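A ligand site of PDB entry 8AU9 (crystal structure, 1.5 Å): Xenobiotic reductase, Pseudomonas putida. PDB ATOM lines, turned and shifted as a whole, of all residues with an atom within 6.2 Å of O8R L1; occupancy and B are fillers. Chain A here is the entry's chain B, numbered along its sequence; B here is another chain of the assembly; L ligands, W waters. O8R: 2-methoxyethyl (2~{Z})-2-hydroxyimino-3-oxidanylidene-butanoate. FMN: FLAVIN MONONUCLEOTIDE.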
ATOM      1  N   PRO A  23      -4.241  32.280 -17.145  1.00  0.00           N
ATOM      2  CA  PRO A  23      -5.328  33.087 -16.571  1.00  0.00           C
ATOM      3  C   PRO A  23      -6.096  32.290 -15.532  1.00  0.00           C
ATOM      4  O   PRO A  23      -6.452  31.136 -15.762  1.00  0.00           O
ATOM      5  CB  PRO A  23      -6.207  33.419 -17.781  1.00  0.00           C
ATOM      6  CG  PRO A  23      -5.843  32.345 -18.830  1.00  0.00           C
ATOM      7  CD  PRO A  23      -4.388  32.101 -18.609  1.00  0.00           C
ATOM      8  N   CYS A  25      -9.320  33.136 -12.997  1.00  0.00           N
ATOM      9  CA  CYS A  25     -10.366  33.977 -12.423  1.00  0.00           C
ATOM     10  C   CYS A  25     -10.293  33.978 -10.906  1.00  0.00           C
ATOM     11  O   CYS A  25     -10.140  32.931 -10.273  1.00  0.00           O
ATOM     12  CB  CYS A  25     -11.737  33.438 -12.824  1.00  0.00           C
ATOM     13  SG  CYS A  25     -12.292  33.928 -14.471  1.00  0.00           S
ATOM     14  N   TYR A  27     -12.769  36.020  -9.115  1.00  0.00           N
ATOM     15  CA  TYR A  27     -14.152  36.275  -8.676  1.00  0.00           C
ATOM     16  C   TYR A  27     -14.227  37.337  -7.581  1.00  0.00           C
ATOM     17  O   TYR A  27     -15.130  37.316  -6.740  1.00  0.00           O
ATOM     18  CB  TYR A  27     -14.859  34.987  -8.244  1.00  0.00           C
ATOM     19  CG  TYR A  27     -14.692  33.835  -9.222  1.00  0.00           C
ATOM     20  CD1 TYR A  27     -15.595  33.644 -10.277  1.00  0.00           C
ATOM     21  CD2 TYR A  27     -13.644  32.943  -9.097  1.00  0.00           C
ATOM     22  CE1 TYR A  27     -15.440  32.588 -11.172  1.00  0.00           C
ATOM     23  CE2 TYR A  27     -13.485  31.878  -9.981  1.00  0.00           C
ATOM     24  CZ  TYR A  27     -14.379  31.713 -11.011  1.00  0.00           C
ATOM     25  OH  TYR A  27     -14.222  30.658 -11.886  1.00  0.00           O
ATOM     26  N   ALA A  57      -9.426  35.699 -17.191  1.00  0.00           N
ATOM     27  CA  ALA A  57     -10.491  36.010 -18.135  1.00  0.00           C
ATOM     28  C   ALA A  57     -11.175  37.320 -17.764  1.00  0.00           C
ATOM     29  O   ALA A  57     -11.802  37.440 -16.708  1.00  0.00           O
ATOM     30  CB  ALA A  57     -11.520  34.887 -18.179  1.00  0.00           C
ATOM     31  N   ILE A  66     -18.401  35.661 -16.411  1.00  0.00           N
ATOM     32  CA  ILE A  66     -18.965  34.413 -15.894  1.00  0.00           C
ATOM     33  C   ILE A  66     -19.895  34.697 -14.726  1.00  0.00           C
ATOM     34  O   ILE A  66     -21.006  34.164 -14.650  1.00  0.00           O
ATOM     35  CB  ILE A  66     -17.846  33.435 -15.486  1.00  0.00           C
ATOM     36  CG1 ILE A  66     -16.840  33.239 -16.625  1.00  0.00           C
ATOM     37  CG2 ILE A  66     -18.442  32.099 -15.056  1.00  0.00           C
ATOM     38  CD1 ILE A  66     -15.640  32.382 -16.213  1.00  0.00           C
ATOM     39  N   GLN A  99      -6.028  37.810 -20.688  1.00  0.00           N
ATOM     40  CA  GLN A  99      -6.977  37.034 -21.467  1.00  0.00           C
ATOM     41  C   GLN A  99      -8.286  37.805 -21.536  1.00  0.00           C
ATOM     42  O   GLN A  99      -8.871  38.126 -20.499  1.00  0.00           O
ATOM     43  CB  GLN A  99      -7.214  35.677 -20.807  1.00  0.00           C
ATOM     44  CG  GLN A  99      -8.088  34.752 -21.653  1.00  0.00           C
ATOM     45  CD  GLN A  99      -8.490  33.507 -20.898  1.00  0.00           C
ATOM     46  OE1 GLN A  99      -9.103  33.591 -19.830  1.00  0.00           O
ATOM     47  NE2 GLN A  99      -8.160  32.338 -21.451  1.00  0.00           N
ATOM     48  N   LYS A 106     -22.312  30.073 -20.532  1.00  0.00           N
ATOM     49  CA  LYS A 106     -21.880  29.800 -19.175  1.00  0.00           C
ATOM     50  C   LYS A 106     -21.900  31.045 -18.282  1.00  0.00           C
ATOM     51  O   LYS A 106     -21.495  30.950 -17.114  1.00  0.00           O
ATOM     52  CB  LYS A 106     -20.481  29.178 -19.178  1.00  0.00           C
ATOM     53  CG  LYS A 106     -20.439  27.807 -19.826  1.00  0.00           C
ATOM     54  CD  LYS A 106     -19.090  27.153 -19.593  1.00  0.00           C
ATOM     55  CE  LYS A 106     -19.078  25.702 -20.033  1.00  0.00           C
ATOM     56  NZ  LYS A 106     -17.780  25.062 -19.651  1.00  0.00           N
ATOM     57  N   HIS A 178      -9.824  34.379 -25.509  1.00  0.00           N
ATOM     58  CA  HIS A 178     -10.354  33.194 -24.832  1.00  0.00           C
ATOM     59  C   HIS A 178     -11.336  32.472 -25.754  1.00  0.00           C
ATOM     60  O   HIS A 178     -12.540  32.735 -25.742  1.00  0.00           O
ATOM     61  CB  HIS A 178     -11.024  33.558 -23.511  1.00  0.00           C
ATOM     62  CG  HIS A 178     -11.206  32.381 -22.615  1.00  0.00           C
ATOM     63  ND1 HIS A 178     -11.028  31.087 -23.049  1.00  0.00           N
ATOM     64  CD2 HIS A 178     -11.529  32.297 -21.300  1.00  0.00           C
ATOM     65  CE1 HIS A 178     -11.239  30.253 -22.045  1.00  0.00           C
ATOM     66  NE2 HIS A 178     -11.542  30.970 -20.966  1.00  0.00           N
ATOM     67  N   ALA A 180     -11.650  29.096 -25.609  1.00  0.00           N
ATOM     68  CA  ALA A 180     -11.632  27.750 -25.043  1.00  0.00           C
ATOM     69  C   ALA A 180     -12.727  27.587 -23.992  1.00  0.00           C
ATOM     70  O   ALA A 180     -13.464  28.510 -23.671  1.00  0.00           O
ATOM     71  CB  ALA A 180     -10.259  27.420 -24.453  1.00  0.00           C
ATOM     72  N   HIS A 181     -12.841  26.354 -23.488  1.00  0.00           N
ATOM     73  CA  HIS A 181     -13.518  26.062 -22.235  1.00  0.00           C
ATOM     74  C   HIS A 181     -15.038  26.231 -22.304  1.00  0.00           C
ATOM     75  O   HIS A 181     -15.681  26.429 -21.265  1.00  0.00           O
ATOM     76  CB  HIS A 181     -12.889  26.845 -21.069  1.00  0.00           C
ATOM     77  CG  HIS A 181     -11.434  26.547 -20.883  1.00  0.00           C
ATOM     78  ND1 HIS A 181     -10.612  27.287 -20.049  1.00  0.00           N
ATOM     79  CD2 HIS A 181     -10.644  25.586 -21.423  1.00  0.00           C
ATOM     80  CE1 HIS A 181      -9.386  26.787 -20.089  1.00  0.00           C
ATOM     81  NE2 HIS A 181      -9.387  25.759 -20.922  1.00  0.00           N
ATOM     82  N   TYR A 183     -16.893  28.571 -23.450  1.00  0.00           N
ATOM     83  CA  TYR A 183     -17.428  29.933 -23.486  1.00  0.00           C
ATOM     84  C   TYR A 183     -17.775  30.323 -24.931  1.00  0.00           C
ATOM     85  O   TYR A 183     -17.928  29.435 -25.785  1.00  0.00           O
ATOM     86  CB  TYR A 183     -16.473  30.896 -22.770  1.00  0.00           C
ATOM     87  CG  TYR A 183     -16.208  30.448 -21.346  1.00  0.00           C
ATOM     88  CD1 TYR A 183     -17.231  30.438 -20.395  1.00  0.00           C
ATOM     89  CD2 TYR A 183     -14.954  29.994 -20.957  1.00  0.00           C
ATOM     90  CE1 TYR A 183     -16.999  30.025 -19.081  1.00  0.00           C
ATOM     91  CE2 TYR A 183     -14.716  29.562 -19.643  1.00  0.00           C
ATOM     92  CZ  TYR A 183     -15.740  29.571 -18.724  1.00  0.00           C
ATOM     93  OH  TYR A 183     -15.495  29.139 -17.431  1.00  0.00           O
ATOM     94  N   ARG A 231      -6.354  30.973 -26.553  1.00  0.00           N
ATOM     95  CA  ARG A 231      -6.551  29.680 -25.917  1.00  0.00           C
ATOM     96  C   ARG A 231      -7.697  28.972 -26.621  1.00  0.00           C
ATOM     97  O   ARG A 231      -8.726  29.587 -26.911  1.00  0.00           O
ATOM     98  CB  ARG A 231      -6.848  29.836 -24.419  1.00  0.00           C
ATOM     99  CG  ARG A 231      -6.793  28.525 -23.659  1.00  0.00           C
ATOM    100  CD  ARG A 231      -6.728  28.723 -22.153  1.00  0.00           C
ATOM    101  NE  ARG A 231      -5.823  27.731 -21.556  1.00  0.00           N
ATOM    102  CZ  ARG A 231      -5.597  27.620 -20.244  1.00  0.00           C
ATOM    103  NH1 ARG A 231      -6.218  28.402 -19.386  1.00  0.00           N
ATOM    104  NH2 ARG A 231      -4.745  26.697 -19.809  1.00  0.00           N
ATOM    105  N   SER A 266      -5.849  23.603 -25.021  1.00  0.00           N
ATOM    106  CA  SER A 266      -6.650  23.192 -23.878  1.00  0.00           C
ATOM    107  C   SER A 266      -7.710  22.191 -24.328  1.00  0.00           C
ATOM    108  O   SER A 266      -7.656  21.646 -25.437  1.00  0.00           O
ATOM    109  CB  SER A 266      -7.230  24.419 -23.157  1.00  0.00           C
ATOM    110  OG  SER A 266      -7.621  24.073 -21.832  1.00  0.00           O
ATOM    111  N   VAL A 267      -8.666  21.925 -23.430  1.00  0.00           N
ATOM    112  CA  VAL A 267      -9.791  21.033 -23.658  1.00  0.00           C
ATOM    113  C   VAL A 267     -11.035  21.890 -23.859  1.00  0.00           C
ATOM    114  O   VAL A 267     -11.106  23.031 -23.385  1.00  0.00           O
ATOM    115  CB  VAL A 267      -9.926  20.078 -22.448  1.00  0.00           C
ATOM    116  CG1 VAL A 267     -11.198  19.244 -22.526  1.00  0.00           C
ATOM    117  CG2 VAL A 267      -8.709  19.163 -22.369  1.00  0.00           C
ATOM    118  N   PHE A 269     -14.427  21.532 -22.955  1.00  0.00           N
ATOM    119  CA  PHE A 269     -15.444  21.708 -21.904  1.00  0.00           C
ATOM    120  C   PHE A 269     -16.754  22.282 -22.450  1.00  0.00           C
ATOM    121  O   PHE A 269     -17.441  23.033 -21.761  1.00  0.00           O
ATOM    122  CB  PHE A 269     -14.922  22.564 -20.739  1.00  0.00           C
ATOM    123  CG  PHE A 269     -13.681  22.049 -20.076  1.00  0.00           C
ATOM    124  CD1 PHE A 269     -13.757  21.056 -19.117  1.00  0.00           C
ATOM    125  CD2 PHE A 269     -12.446  22.586 -20.377  1.00  0.00           C
ATOM    126  CE1 PHE A 269     -12.622  20.601 -18.474  1.00  0.00           C
ATOM    127  CE2 PHE A 269     -11.304  22.133 -19.746  1.00  0.00           C
ATOM    128  CZ  PHE A 269     -11.388  21.126 -18.794  1.00  0.00           C
ATOM    129  N   TRP A 278      -7.969  12.836 -16.712  1.00  0.00           N
ATOM    130  CA  TRP A 278      -7.090  13.636 -15.873  1.00  0.00           C
ATOM    131  C   TRP A 278      -5.896  12.801 -15.402  1.00  0.00           C
ATOM    132  O   TRP A 278      -6.037  11.623 -15.063  1.00  0.00           O
ATOM    133  CB  TRP A 278      -7.848  14.125 -14.644  1.00  0.00           C
ATOM    134  CG  TRP A 278      -9.072  14.907 -14.973  1.00  0.00           C
ATOM    135  CD1 TRP A 278     -10.362  14.511 -14.842  1.00  0.00           C
ATOM    136  CD2 TRP A 278      -9.108  16.239 -15.494  1.00  0.00           C
ATOM    137  NE1 TRP A 278     -11.219  15.508 -15.244  1.00  0.00           N
ATOM    138  CE2 TRP A 278     -10.477  16.588 -15.648  1.00  0.00           C
ATOM    139  CE3 TRP A 278      -8.133  17.174 -15.858  1.00  0.00           C
ATOM    140  CZ2 TRP A 278     -10.872  17.818 -16.151  1.00  0.00           C
ATOM    141  CZ3 TRP A 278      -8.536  18.403 -16.349  1.00  0.00           C
ATOM    142  CH2 TRP A 278      -9.900  18.711 -16.490  1.00  0.00           C
ATOM    143  N   TRP A 302      -2.974  21.891 -17.028  1.00  0.00           N
ATOM    144  CA  TRP A 302      -3.761  20.772 -16.530  1.00  0.00           C
ATOM    145  C   TRP A 302      -2.889  19.603 -16.101  1.00  0.00           C
ATOM    146  O   TRP A 302      -3.117  18.465 -16.528  1.00  0.00           O
ATOM    147  CB  TRP A 302      -4.821  20.294 -17.528  1.00  0.00           C
ATOM    148  CG  TRP A 302      -5.685  21.396 -18.073  1.00  0.00           C
ATOM    149  CD1 TRP A 302      -5.559  22.022 -19.285  1.00  0.00           C
ATOM    150  CD2 TRP A 302      -6.804  22.010 -17.411  1.00  0.00           C
ATOM    151  NE1 TRP A 302      -6.535  22.988 -19.419  1.00  0.00           N
ATOM    152  CE2 TRP A 302      -7.314  22.992 -18.285  1.00  0.00           C
ATOM    153  CE3 TRP A 302      -7.426  21.806 -16.177  1.00  0.00           C
ATOM    154  CZ2 TRP A 302      -8.414  23.791 -17.953  1.00  0.00           C
ATOM    155  CZ3 TRP A 302      -8.517  22.608 -15.846  1.00  0.00           C
ATOM    156  CH2 TRP A 302      -9.005  23.575 -16.742  1.00  0.00           C
ATOM    157  N   TRP B 358     -10.084  25.922  -4.714  1.00  0.00           N
ATOM    158  CA  TRP B 358      -9.469  25.135  -5.775  1.00  0.00           C
ATOM    159  C   TRP B 358      -8.419  24.174  -5.255  1.00  0.00           C
ATOM    160  O   TRP B 358      -8.162  23.135  -5.873  1.00  0.00           O
ATOM    161  CB  TRP B 358      -8.848  26.076  -6.796  1.00  0.00           C
ATOM    162  CG  TRP B 358      -9.849  27.044  -7.273  1.00  0.00           C
ATOM    163  CD1 TRP B 358     -10.031  28.316  -6.837  1.00  0.00           C
ATOM    164  CD2 TRP B 358     -10.849  26.796  -8.256  1.00  0.00           C
ATOM    165  NE1 TRP B 358     -11.099  28.896  -7.494  1.00  0.00           N
ATOM    166  CE2 TRP B 358     -11.611  27.977  -8.378  1.00  0.00           C
ATOM    167  CE3 TRP B 358     -11.182  25.698  -9.047  1.00  0.00           C
ATOM    168  CZ2 TRP B 358     -12.671  28.094  -9.270  1.00  0.00           C
ATOM    169  CZ3 TRP B 358     -12.232  25.817  -9.941  1.00  0.00           C
ATOM    170  CH2 TRP B 358     -12.971  27.007 -10.037  1.00  0.00           C
HETATM  171  N1  O8R L   1     -12.126  29.494 -17.424  1.00  0.00           N
HETATM  172  C4  O8R L   1     -11.855  27.094 -17.024  1.00  0.00           C
HETATM  173  C5  O8R L   1     -12.327  25.027 -18.010  1.00  0.00           C
HETATM  174  C6  O8R L   1     -12.773  24.017 -16.958  1.00  0.00           C
HETATM  175  C7  O8R L   1     -14.727  23.105 -16.021  1.00  0.00           C
HETATM  176  C1  O8R L   1     -13.355  27.546 -14.489  1.00  0.00           C
HETATM  177  C2  O8R L   1     -12.926  28.764 -15.307  1.00  0.00           C
HETATM  178  C3  O8R L   1     -12.275  28.518 -16.648  1.00  0.00           C
HETATM  179  O1  O8R L   1     -13.115  29.884 -14.923  1.00  0.00           O
HETATM  180  O2  O8R L   1     -10.774  26.661 -16.783  1.00  0.00           O
HETATM  181  O3  O8R L   1     -12.797  26.287 -17.658  1.00  0.00           O
HETATM  182  O4  O8R L   1     -11.537  29.308 -18.670  1.00  0.00           O
HETATM  183  O5  O8R L   1     -14.156  24.152 -16.760  1.00  0.00           O
HETATM  184  N1  FMN L   2      -8.497  29.210 -17.672  1.00  0.00           N
HETATM  185  C2  FMN L   2      -8.821  30.210 -18.547  1.00  0.00           C
HETATM  186  O2  FMN L   2      -8.621  30.041 -19.743  1.00  0.00           O
HETATM  187  N3  FMN L   2      -9.339  31.408 -18.099  1.00  0.00           N
HETATM  188  C4  FMN L   2      -9.566  31.619 -16.761  1.00  0.00           C
HETATM  189  O4  FMN L   2     -10.012  32.691 -16.351  1.00  0.00           O
HETATM  190  C4A FMN L   2      -9.238  30.611 -15.875  1.00  0.00           C
HETATM  191  N5  FMN L   2      -9.459  30.803 -14.536  1.00  0.00           N
HETATM  192  C5A FMN L   2      -9.113  29.811 -13.645  1.00  0.00           C
HETATM  193  C6  FMN L   2      -9.334  30.046 -12.290  1.00  0.00           C
HETATM  194  C7  FMN L   2      -9.000  29.085 -11.360  1.00  0.00           C
HETATM  195  C7M FMN L   2      -9.221  29.389  -9.901  1.00  0.00           C
HETATM  196  C8  FMN L   2      -8.463  27.884 -11.770  1.00  0.00           C
HETATM  197  C8M FMN L   2      -8.106  26.831 -10.751  1.00  0.00           C
HETATM  198  C9  FMN L   2      -8.250  27.636 -13.132  1.00  0.00           C
HETATM  199  C9A FMN L   2      -8.570  28.611 -14.077  1.00  0.00           C
HETATM  200  N10 FMN L   2      -8.382  28.408 -15.440  1.00  0.00           N
HETATM  201  C10 FMN L   2      -8.698  29.409 -16.327  1.00  0.00           C
HETATM  202  C1' FMN L   2      -7.756  27.146 -15.929  1.00  0.00           C
HETATM  203  C2' FMN L   2      -6.241  27.385 -15.691  1.00  0.00           C
HETATM  204  O2' FMN L   2      -5.753  28.442 -16.510  1.00  0.00           O
HETATM  205  C3' FMN L   2      -5.406  26.132 -15.909  1.00  0.00           C
HETATM  206  O3' FMN L   2      -5.618  25.669 -17.219  1.00  0.00           O
HETATM  207  C4' FMN L   2      -5.799  25.040 -14.928  1.00  0.00           C
HETATM  208  O4' FMN L   2      -5.713  25.517 -13.589  1.00  0.00           O
HETATM  209  C5' FMN L   2      -4.909  23.807 -15.106  1.00  0.00           C
HETATM  210  O5' FMN L   2      -3.548  24.071 -14.856  1.00  0.00           O
HETATM  211  P   FMN L   2      -2.852  23.608 -13.480  1.00  0.00           P
HETATM  212  O1P FMN L   2      -3.651  24.266 -12.365  1.00  0.00           O
HETATM  213  O2P FMN L   2      -1.424  24.064 -13.517  1.00  0.00           O
HETATM  214  O3P FMN L   2      -2.970  22.105 -13.414  1.00  0.00           O
HETATM  215  O   HOH W   1     -15.839  26.256 -17.826  1.00  0.00           O
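OH of Tyr 27 lies within hydrogen-bond range of O1 of O8R L1 (3.3 Å). N of Cys 25 is in hydrogen-bond range of N5 of FMN L2 (2.8 Å). NE2 of His 178 sits at hydrogen-bond distance from O2 of FMN L2, 3.3 Å away. An oxygen (O4) of O8R L1 is in hydrogen-bond range of a ring nitrogen (ND1) of His 181 (2.6 Å). OH of Tyr 183 sits close to N1 of O8R L1 (3.4 Å). The backbone NH of Trp 302 sits at hydrogen-bond distance from an oxygen (O5') of FMN L2, at 3.1 Å. The side-chain amide oxygen (OE1) of Gln 99 sits at hydrogen-bond distance from a nitrogen (N3) of FMN L2 (2.8 Å). An oxygen (O2') of FMN L2 lies within hydrogen-bond range of the guanidinium group of Arg 231 (2.9 Å). O of Pro 23 lies close to O2' of FMN L2 (2.9 Å). ND1 of His 181 lies close to O2 of FMN L2 (3.4 Å). A ring nitrogen (NE2) of His 178 sits at hydrogen-bond distance from an oxygen (O4) of O8R L1, at 2.8 Å. The backbone NH (N) of Ala 57 sits at hydrogen-bond distance from an oxygen (O4) of FMN L2, 3.2 Å away. SG of Cys 25 is in hydrogen-bond range of O4 of FMN L2 (3.2 Å).
Ile 66 touches O8R L1 (CD1 to O1, 3.8 Å). CD2 of Phe 269 touches C5 of O8R L1 (3.4 Å). Trp 302 touches O8R L1. Hydrophobic or aromatic side chains that line O8R L1: Ile 66, His 178, His 181, Tyr 183, Phe 269 and Trp 302.
O of Phe 269 lies within hydrogen-bond range of NZ of Lys 106 (2.9 Å). A ring nitrogen (NE2) of His 181 is in hydrogen-bond range of the side-chain hydroxyl (OG) of Ser 266, at 2.6 Å. NE1 of Trp 302 is in hydrogen-bond range of OG of Ser 266, 2.9 Å away. The side-chain amino group (NZ) of Lys 106 lies within hydrogen-bond range of the backbone carbonyl oxygen (O) of His 181, at 3.0 Å. The backbone NH (N) of Ala 180 lies within hydrogen-bond range of a ring nitrogen (ND1) of His 178 (3.3 Å).
O4 of O8R L1 sits close to N3 of FMN L2 (3.1 Å).
Water W1 lies within hydrogen-bond range of an oxygen (O5) of O8R L1 (2.9 Å), the side-chain amino group of Lys 106 (2.9 Å), the side-chain hydroxyl of Tyr 183 (2.9 Å) and the backbone carbonyl oxygen of His 181 (3.4 Å).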
